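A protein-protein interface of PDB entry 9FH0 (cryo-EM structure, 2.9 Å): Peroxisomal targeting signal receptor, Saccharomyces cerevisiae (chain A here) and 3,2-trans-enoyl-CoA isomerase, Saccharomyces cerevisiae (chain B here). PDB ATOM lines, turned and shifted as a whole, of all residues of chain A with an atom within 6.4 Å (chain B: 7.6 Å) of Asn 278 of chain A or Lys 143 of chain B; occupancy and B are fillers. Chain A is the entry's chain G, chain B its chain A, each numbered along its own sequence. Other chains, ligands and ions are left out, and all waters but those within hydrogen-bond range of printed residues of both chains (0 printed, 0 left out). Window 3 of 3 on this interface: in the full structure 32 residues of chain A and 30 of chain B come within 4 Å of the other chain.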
ATOM      1  N   LEU A 276       9.516  13.400  15.085  1.00  0.00           N
ATOM      2  CA  LEU A 276       8.827  14.248  16.050  1.00  0.00           C
ATOM      3  C   LEU A 276       9.545  15.576  16.245  1.00  0.00           C
ATOM      4  O   LEU A 276       9.167  16.368  17.104  1.00  0.00           O
ATOM      5  CB  LEU A 276       8.696  13.540  17.396  1.00  0.00           C
ATOM      6  CG  LEU A 276       7.550  12.558  17.590  1.00  0.00           C
ATOM      7  CD1 LEU A 276       7.896  11.218  16.978  1.00  0.00           C
ATOM      8  CD2 LEU A 276       7.242  12.417  19.062  1.00  0.00           C
ATOM      9  N   VAL A 277      10.583  15.814  15.461  1.00  0.00           N
ATOM     10  CA  VAL A 277      11.343  17.053  15.536  1.00  0.00           C
ATOM     11  C   VAL A 277      10.906  17.955  14.394  1.00  0.00           C
ATOM     12  O   VAL A 277      10.576  17.481  13.303  1.00  0.00           O
ATOM     13  CB  VAL A 277      12.860  16.780  15.500  1.00  0.00           C
ATOM     14  CG1 VAL A 277      13.294  16.320  14.130  1.00  0.00           C
ATOM     15  CG2 VAL A 277      13.640  18.007  15.924  1.00  0.00           C
ATOM     16  N   ASN A 278      10.856  19.258  14.659  1.00  0.00           N
ATOM     17  CA  ASN A 278      10.527  20.234  13.628  1.00  0.00           C
ATOM     18  C   ASN A 278      11.797  20.841  13.048  1.00  0.00           C
ATOM     19  O   ASN A 278      11.994  20.853  11.831  1.00  0.00           O
ATOM     20  CB  ASN A 278       9.621  21.324  14.204  1.00  0.00           C
ATOM     21  CG  ASN A 278       8.943  22.143  13.133  1.00  0.00           C
ATOM     22  OD1 ASN A 278       9.517  23.079  12.591  1.00  0.00           O
ATOM     23  ND2 ASN A 278       7.709  21.800  12.829  1.00  0.00           N
ATOM     24  N   ASP A 279      12.666  21.333  13.916  1.00  0.00           N
ATOM     25  CA  ASP A 279      13.934  21.950  13.552  1.00  0.00           C
ATOM     26  C   ASP A 279      14.730  22.119  14.835  1.00  0.00           C
ATOM     27  O   ASP A 279      14.246  21.818  15.930  1.00  0.00           O
ATOM     28  CB  ASP A 279      13.727  23.292  12.859  1.00  0.00           C
ATOM     29  CG  ASP A 279      12.810  24.195  13.628  1.00  0.00           C
ATOM     30  OD1 ASP A 279      11.753  23.721  14.060  1.00  0.00           O
ATOM     31  OD2 ASP A 279      13.141  25.374  13.826  1.00  0.00           O
ATOM     32  N   ASP A 280      15.962  22.589  14.697  1.00  0.00           N
ATOM     33  CA  ASP A 280      16.595  23.222  15.837  1.00  0.00           C
ATOM     34  C   ASP A 280      15.953  24.584  16.029  1.00  0.00           C
ATOM     35  O   ASP A 280      15.504  25.212  15.072  1.00  0.00           O
ATOM     36  CB  ASP A 280      18.106  23.349  15.640  1.00  0.00           C
ATOM     37  CG  ASP A 280      18.475  23.951  14.305  1.00  0.00           C
ATOM     38  N   ASN A 282      13.153  24.753  17.578  1.00  0.00           N
ATOM     39  CA  ASN A 282      11.888  24.208  18.085  1.00  0.00           C
ATOM     40  C   ASN A 282      10.707  25.174  17.954  1.00  0.00           C
ATOM     41  O   ASN A 282      10.036  25.500  18.930  1.00  0.00           O
ATOM     42  CB  ASN A 282      12.064  23.778  19.542  1.00  0.00           C
ATOM     43  CG  ASN A 282      10.847  23.072  20.103  1.00  0.00           C
ATOM     44  OD1 ASN A 282      10.037  22.508  19.369  1.00  0.00           O
ATOM     45  ND2 ASN A 282      10.711  23.109  21.418  1.00  0.00           N
ATOM     46  N   LEU A 283      10.434  25.606  16.724  1.00  0.00           N
ATOM     47  CA  LEU A 283       9.281  26.458  16.432  1.00  0.00           C
ATOM     48  C   LEU A 283       9.275  27.715  17.289  1.00  0.00           C
ATOM     49  O   LEU A 283       8.296  28.029  17.962  1.00  0.00           O
ATOM     50  CB  LEU A 283       7.980  25.691  16.619  1.00  0.00           C
ATOM     51  CG  LEU A 283       7.452  24.863  15.466  1.00  0.00           C
ATOM     52  CD1 LEU A 283       6.501  23.811  15.968  1.00  0.00           C
ATOM     53  CD2 LEU A 283       6.731  25.787  14.541  1.00  0.00           C
ATOM     54  N   ASP A 423      15.357  10.570   9.483  1.00  0.00           N
ATOM     55  CA  ASP A 423      14.456  11.709   9.646  1.00  0.00           C
ATOM     56  C   ASP A 423      13.468  11.462  10.777  1.00  0.00           C
ATOM     57  O   ASP A 423      12.293  11.194  10.533  1.00  0.00           O
ATOM     58  CB  ASP A 423      13.696  12.008   8.350  1.00  0.00           C
ATOM     59  CG  ASP A 423      14.606  12.104   7.152  1.00  0.00           C
ATOM     60  OD1 ASP A 423      15.824  12.262   7.354  1.00  0.00           O
ATOM     61  OD2 ASP A 423      14.103  12.035   6.010  1.00  0.00           O
ATOM     62  N   THR A 433       7.282  17.962  15.372  1.00  0.00           N
ATOM     63  CA  THR A 433       6.955  19.256  15.955  1.00  0.00           C
ATOM     64  C   THR A 433       6.797  19.135  17.463  1.00  0.00           C
ATOM     65  O   THR A 433       6.331  20.054  18.126  1.00  0.00           O
ATOM     66  CB  THR A 433       5.681  19.815  15.354  1.00  0.00           C
ATOM     67  OG1 THR A 433       4.555  19.241  16.023  1.00  0.00           O
ATOM     68  CG2 THR A 433       5.614  19.452  13.887  1.00  0.00           C
ATOM     69  N   HIS A 434       7.203  17.984  17.991  1.00  0.00           N
ATOM     70  CA  HIS A 434       7.066  17.658  19.401  1.00  0.00           C
ATOM     71  C   HIS A 434       8.384  17.711  20.160  1.00  0.00           C
ATOM     72  O   HIS A 434       8.396  18.036  21.350  1.00  0.00           O
ATOM     73  CB  HIS A 434       6.464  16.260  19.554  1.00  0.00           C
ATOM     74  CG  HIS A 434       5.041  16.156  19.114  1.00  0.00           C
ATOM     75  ND1 HIS A 434       4.557  15.070  18.417  1.00  0.00           N
ATOM     76  CD2 HIS A 434       3.988  16.986  19.293  1.00  0.00           C
ATOM     77  CE1 HIS A 434       3.270  15.240  18.175  1.00  0.00           C
ATOM     78  NE2 HIS A 434       2.900  16.396  18.697  1.00  0.00           N
ATOM     79  N   ILE A 435       9.491  17.399  19.502  1.00  0.00           N
ATOM     80  CA  ILE A 435      10.772  17.176  20.155  1.00  0.00           C
ATOM     81  C   ILE A 435      11.678  18.377  19.924  1.00  0.00           C
ATOM     82  O   ILE A 435      11.625  19.027  18.875  1.00  0.00           O
ATOM     83  CB  ILE A 435      11.385  15.863  19.622  1.00  0.00           C
ATOM     84  CG1 ILE A 435      10.774  14.667  20.341  1.00  0.00           C
ATOM     85  CG2 ILE A 435      12.875  15.827  19.762  1.00  0.00           C
ATOM     86  CD1 ILE A 435      11.359  13.356  19.905  1.00  0.00           C
ATOM     87  N   ARG B  64      19.634  24.417   6.915  1.00  0.00           N
ATOM     88  CA  ARG B  64      18.334  24.096   7.465  1.00  0.00           C
ATOM     89  C   ARG B  64      17.529  25.317   7.867  1.00  0.00           C
ATOM     90  O   ARG B  64      16.359  25.176   8.206  1.00  0.00           O
ATOM     91  CB  ARG B  64      18.491  23.182   8.678  1.00  0.00           C
ATOM     92  CG  ARG B  64      19.231  21.908   8.385  1.00  0.00           C
ATOM     93  CD  ARG B  64      18.368  20.721   8.680  1.00  0.00           C
ATOM     94  NE  ARG B  64      19.033  19.471   8.352  1.00  0.00           N
ATOM     95  CZ  ARG B  64      18.476  18.275   8.500  1.00  0.00           C
ATOM     96  NH1 ARG B  64      17.242  18.171   8.972  1.00  0.00           N
ATOM     97  NH2 ARG B  64      19.150  17.179   8.177  1.00  0.00           N
ATOM     98  N   ASN B 120      13.929  27.566   2.413  1.00  0.00           N
ATOM     99  CA  ASN B 120      14.419  26.234   2.722  1.00  0.00           C
ATOM    100  C   ASN B 120      14.287  25.896   4.189  1.00  0.00           C
ATOM    101  O   ASN B 120      14.577  24.767   4.579  1.00  0.00           O
ATOM    102  CB  ASN B 120      15.870  26.089   2.301  1.00  0.00           C
ATOM    103  CG  ASN B 120      16.749  27.030   3.010  1.00  0.00           C
ATOM    104  OD1 ASN B 120      16.503  28.217   3.010  1.00  0.00           O
ATOM    105  ND2 ASN B 120      17.778  26.520   3.638  1.00  0.00           N
ATOM    106  N   GLY B 121      13.846  26.833   5.002  1.00  0.00           N
ATOM    107  CA  GLY B 121      13.678  26.605   6.406  1.00  0.00           C
ATOM    108  C   GLY B 121      13.098  27.836   7.036  1.00  0.00           C
ATOM    109  O   GLY B 121      12.637  28.739   6.350  1.00  0.00           O
ATOM    110  N   PRO B 122      13.112  27.903   8.355  1.00  0.00           N
ATOM    111  CA  PRO B 122      12.540  29.056   9.042  1.00  0.00           C
ATOM    112  C   PRO B 122      13.309  30.337   8.781  1.00  0.00           C
ATOM    113  O   PRO B 122      14.473  30.332   8.400  1.00  0.00           O
ATOM    114  CB  PRO B 122      12.633  28.653  10.505  1.00  0.00           C
ATOM    115  CG  PRO B 122      12.674  27.213  10.472  1.00  0.00           C
ATOM    116  CD  PRO B 122      13.394  26.807   9.280  1.00  0.00           C
ATOM    117  N   SER B 139       8.159  27.201  -0.612  1.00  0.00           N
ATOM    118  CA  SER B 139       8.678  26.548   0.572  1.00  0.00           C
ATOM    119  C   SER B 139       9.153  25.154   0.217  1.00  0.00           C
ATOM    120  O   SER B 139       8.678  24.550  -0.739  1.00  0.00           O
ATOM    121  CB  SER B 139       7.638  26.468   1.655  1.00  0.00           C
ATOM    122  OG  SER B 139       6.544  25.713   1.219  1.00  0.00           O
ATOM    123  N   ILE B 140      10.102  24.646   0.997  1.00  0.00           N
ATOM    124  CA  ILE B 140      10.656  23.332   0.712  1.00  0.00           C
ATOM    125  C   ILE B 140       9.747  22.241   1.240  1.00  0.00           C
ATOM    126  O   ILE B 140       9.450  21.278   0.536  1.00  0.00           O
ATOM    127  CB  ILE B 140      12.080  23.220   1.275  1.00  0.00           C
ATOM    128  CG1 ILE B 140      12.661  21.847   1.005  1.00  0.00           C
ATOM    129  CG2 ILE B 140      12.109  23.521   2.728  1.00  0.00           C
ATOM    130  CD1 ILE B 140      14.093  21.773   1.332  1.00  0.00           C
ATOM    131  N   ASN B 141       9.272  22.384   2.468  1.00  0.00           N
ATOM    132  CA  ASN B 141       8.288  21.481   3.028  1.00  0.00           C
ATOM    133  C   ASN B 141       7.428  22.291   3.984  1.00  0.00           C
ATOM    134  O   ASN B 141       7.415  23.521   3.928  1.00  0.00           O
ATOM    135  CB  ASN B 141       8.959  20.265   3.681  1.00  0.00           C
ATOM    136  CG  ASN B 141      10.157  20.627   4.499  1.00  0.00           C
ATOM    137  OD1 ASN B 141      10.223  21.690   5.087  1.00  0.00           O
ATOM    138  ND2 ASN B 141      11.125  19.740   4.538  1.00  0.00           N
ATOM    139  N   ASP B 142       6.692  21.610   4.854  1.00  0.00           N
ATOM    140  CA  ASP B 142       5.732  22.259   5.728  1.00  0.00           C
ATOM    141  C   ASP B 142       6.262  22.459   7.131  1.00  0.00           C
ATOM    142  O   ASP B 142       5.488  22.505   8.085  1.00  0.00           O
ATOM    143  CB  ASP B 142       4.447  21.454   5.774  1.00  0.00           C
ATOM    144  CG  ASP B 142       4.701  20.013   5.968  1.00  0.00           C
ATOM    145  OD1 ASP B 142       5.555  19.478   5.245  1.00  0.00           O
ATOM    146  OD2 ASP B 142       4.061  19.408   6.844  1.00  0.00           O
ATOM    147  N   LYS B 143       7.567  22.579   7.282  1.00  0.00           N
ATOM    148  CA  LYS B 143       8.163  22.814   8.581  1.00  0.00           C
ATOM    149  C   LYS B 143       8.754  24.204   8.671  1.00  0.00           C
ATOM    150  O   LYS B 143       9.544  24.482   9.570  1.00  0.00           O
ATOM    151  CB  LYS B 143       9.215  21.752   8.866  1.00  0.00           C
ATOM    152  CG  LYS B 143       8.643  20.364   8.869  1.00  0.00           C
ATOM    153  CD  LYS B 143       9.567  19.377   9.529  1.00  0.00           C
ATOM    154  CE  LYS B 143      10.236  18.483   8.519  1.00  0.00           C
ATOM    155  NZ  LYS B 143      10.858  17.306   9.168  1.00  0.00           N
ATOM    156  N   VAL B 144       8.399  25.051   7.778  1.00  0.00           N
ATOM    157  CA  VAL B 144       8.900  26.410   7.726  1.00  0.00           C
ATOM    158  C   VAL B 144       7.978  27.290   8.548  1.00  0.00           C
ATOM    159  O   VAL B 144       6.798  26.996   8.715  1.00  0.00           O
ATOM    160  CB  VAL B 144       9.001  26.873   6.263  1.00  0.00           C
ATOM    161  CG1 VAL B 144       9.752  25.864   5.462  1.00  0.00           C
ATOM    162  CG2 VAL B 144       7.642  27.043   5.679  1.00  0.00           C
ATOM    163  N   TYR B 145       8.516  28.371   9.092  1.00  0.00           N
ATOM    164  CA  TYR B 145       7.709  29.311   9.851  1.00  0.00           C
ATOM    165  C   TYR B 145       8.420  30.649   9.835  1.00  0.00           C
ATOM    166  O   TYR B 145       9.550  30.763   9.369  1.00  0.00           O
ATOM    167  CB  TYR B 145       7.457  28.817  11.275  1.00  0.00           C
ATOM    168  CG  TYR B 145       8.690  28.614  12.109  1.00  0.00           C
ATOM    169  CD1 TYR B 145       9.238  29.647  12.821  1.00  0.00           C
ATOM    170  CD2 TYR B 145       9.294  27.387  12.194  1.00  0.00           C
ATOM    171  CE1 TYR B 145      10.351  29.472  13.568  1.00  0.00           C
ATOM    172  CE2 TYR B 145      10.404  27.207  12.944  1.00  0.00           C
ATOM    173  CZ  TYR B 145      10.930  28.253  13.628  1.00  0.00           C
ATOM    174  OH  TYR B 145      12.051  28.077  14.390  1.00  0.00           O
ATOM    175  N   LEU B 146       7.732  31.671  10.320  1.00  0.00           N
ATOM    176  CA  LEU B 146       8.299  33.001  10.452  1.00  0.00           C
ATOM    177  C   LEU B 146       8.122  33.439  11.890  1.00  0.00           C
ATOM    178  O   LEU B 146       7.040  33.289  12.452  1.00  0.00           O
ATOM    179  CB  LEU B 146       7.625  34.001   9.523  1.00  0.00           C
ATOM    180  CG  LEU B 146       7.385  33.716   8.049  1.00  0.00           C
ATOM    181  CD1 LEU B 146       6.471  34.765   7.495  1.00  0.00           C
ATOM    182  CD2 LEU B 146       8.666  33.717   7.294  1.00  0.00           C
ATOM    183  N   LYS B 185       3.134  29.970  11.779  1.00  0.00           N
ATOM    184  CA  LYS B 185       3.403  28.605  11.371  1.00  0.00           C
ATOM    185  C   LYS B 185       2.957  28.381   9.938  1.00  0.00           C
ATOM    186  O   LYS B 185       2.435  29.267   9.276  1.00  0.00           O
ATOM    187  CB  LYS B 185       2.704  27.628  12.299  1.00  0.00           C
ATOM    188  CG  LYS B 185       3.290  27.564  13.661  1.00  0.00           C
ATOM    189  CD  LYS B 185       2.492  26.635  14.507  1.00  0.00           C
ATOM    190  CE  LYS B 185       3.082  26.538  15.881  1.00  0.00           C
ATOM    191  NZ  LYS B 185       2.309  25.589  16.718  1.00  0.00           N
ATOM    192  N   TYR B 186       3.154  27.162   9.456  1.00  0.00           N
ATOM    193  CA  TYR B 186       2.937  26.909   8.042  1.00  0.00           C
ATOM    194  C   TYR B 186       1.467  26.868   7.685  1.00  0.00           C
ATOM    195  O   TYR B 186       1.100  27.239   6.572  1.00  0.00           O
ATOM    196  CB  TYR B 186       3.606  25.612   7.639  1.00  0.00           C
ATOM    197  CG  TYR B 186       3.231  25.124   6.274  1.00  0.00           C
ATOM    198  CD1 TYR B 186       3.810  25.653   5.147  1.00  0.00           C
ATOM    199  CD2 TYR B 186       2.316  24.113   6.116  1.00  0.00           C
ATOM    200  CE1 TYR B 186       3.473  25.203   3.913  1.00  0.00           C
ATOM    201  CE2 TYR B 186       1.985  23.657   4.887  1.00  0.00           C
ATOM    202  CZ  TYR B 186       2.566  24.201   3.795  1.00  0.00           C
ATOM    203  OH  TYR B 186       2.214  23.736   2.564  1.00  0.00           O
ATOM    204  N   MET B 189       0.265  30.211   7.076  1.00  0.00           N
ATOM    205  CA  MET B 189       0.765  30.646   5.782  1.00  0.00           C
ATOM    206  C   MET B 189      -0.064  30.073   4.649  1.00  0.00           C
ATOM    207  O   MET B 189      -0.264  30.739   3.636  1.00  0.00           O
ATOM    208  CB  MET B 189       2.233  30.248   5.656  1.00  0.00           C
ATOM    209  CG  MET B 189       3.113  31.001   6.622  1.00  0.00           C
ATOM    210  SD  MET B 189       4.734  30.321   6.993  1.00  0.00           S
ATOM    211  CE  MET B 189       5.630  30.637   5.522  1.00  0.00           C
ATOM    212  N   ASN B 198       4.337  24.356  -2.423  1.00  0.00           N
ATOM    213  CA  ASN B 198       5.083  23.602  -1.423  1.00  0.00           C
ATOM    214  C   ASN B 198       5.732  22.422  -2.130  1.00  0.00           C
ATOM    215  O   ASN B 198       5.039  21.513  -2.589  1.00  0.00           O
ATOM    216  CB  ASN B 198       4.152  23.142  -0.309  1.00  0.00           C
ATOM    217  CG  ASN B 198       4.839  22.312   0.710  1.00  0.00           C
ATOM    218  OD1 ASN B 198       6.028  22.413   0.889  1.00  0.00           O
ATOM    219  ND2 ASN B 198       4.090  21.486   1.401  1.00  0.00           N
ATOM    220  N   MET B 201       9.926  18.461  -0.036  1.00  0.00           N
ATOM    221  CA  MET B 201      11.197  17.786  -0.203  1.00  0.00           C
ATOM    222  C   MET B 201      11.778  17.459   1.162  1.00  0.00           C
ATOM    223  O   MET B 201      11.304  17.991   2.170  1.00  0.00           O
ATOM    224  CB  MET B 201      12.146  18.665  -1.000  1.00  0.00           C
ATOM    225  CG  MET B 201      11.946  18.555  -2.473  1.00  0.00           C
ATOM    226  SD  MET B 201      13.012  19.654  -3.375  1.00  0.00           S
ATOM    227  CE  MET B 201      12.984  18.867  -4.961  1.00  0.00           C
ATOM    228  N   PRO B 202      12.770  16.578   1.251  1.00  0.00           N
ATOM    229  CA  PRO B 202      13.437  16.370   2.535  1.00  0.00           C
ATOM    230  C   PRO B 202      14.182  17.622   2.947  1.00  0.00           C
ATOM    231  O   PRO B 202      14.836  18.270   2.132  1.00  0.00           O
ATOM    232  CB  PRO B 202      14.397  15.215   2.251  1.00  0.00           C
ATOM    233  CG  PRO B 202      13.864  14.568   1.056  1.00  0.00           C
ATOM    234  CD  PRO B 202      13.266  15.640   0.236  1.00  0.00           C
ATOM    235  N   SER B 203      14.078  17.959   4.222  1.00  0.00           N
ATOM    236  CA  SER B 203      14.632  19.220   4.684  1.00  0.00           C
ATOM    237  C   SER B 203      16.141  19.247   4.691  1.00  0.00           C
ATOM    238  O   SER B 203      16.708  20.275   5.055  1.00  0.00           O
ATOM    239  CB  SER B 203      14.126  19.533   6.084  1.00  0.00           C
ATOM    240  OG  SER B 203      14.807  20.658   6.592  1.00  0.00           O
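Among the printed residues, pairs that only touch across the chains: Asp 279 of chain A with Pro 122 of chain B (3.9 Å), Leu 283 of chain A with Tyr 145 of chain B (3.7 Å) and Leu 283 of chain A with Lys 185 of chain B (3.96 Å).
Of the 11 printed residues of chain A, 3 touch a printed residue of chain B.
Hydrophobic or aromatic side chains of chain A within 4 Å of the printed part of chain B: Leu 283.
Hydrophobic or aromatic side chains of chain B that line the printed part of chain A: Pro 122 and Tyr 145.
Among the printed residues, 5 pairs touch across the chains.
The side-chain amide oxygen (OD1) of Asn 278 of chain A lies close to the side-chain carboxylate (OD1) of Asp 279 of chain A.
Of the printed residues of chain B, Asp 279 of chain A touches Pro 122 (3.9 Å) and Tyr 145 (3.0 Å).
Of the printed residues of chain B, Leu 283 of chain A touches Tyr 145 and Lys 185.
Asp 423 of chain A touches none of the printed residues of chain B.
Of the printed residues of chain A, Pro 122 of chain B touches Asp 279 (3.9 Å).
Printed residues of chain A within 4 Å of Tyr 145 of chain B: Asp 279 (3.0 Å) and Leu 283 (3.7 Å).
The side-chain amide oxygen (OD1) of Asn 278 of chain A lies close to the backbone carbonyl oxygen (O) of Lys 143 of chain B (3.3 Å).
OH of Tyr 145 of chain B sits at hydrogen-bond distance from OD2 of Asp 279 of chain A (3.0 Å).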
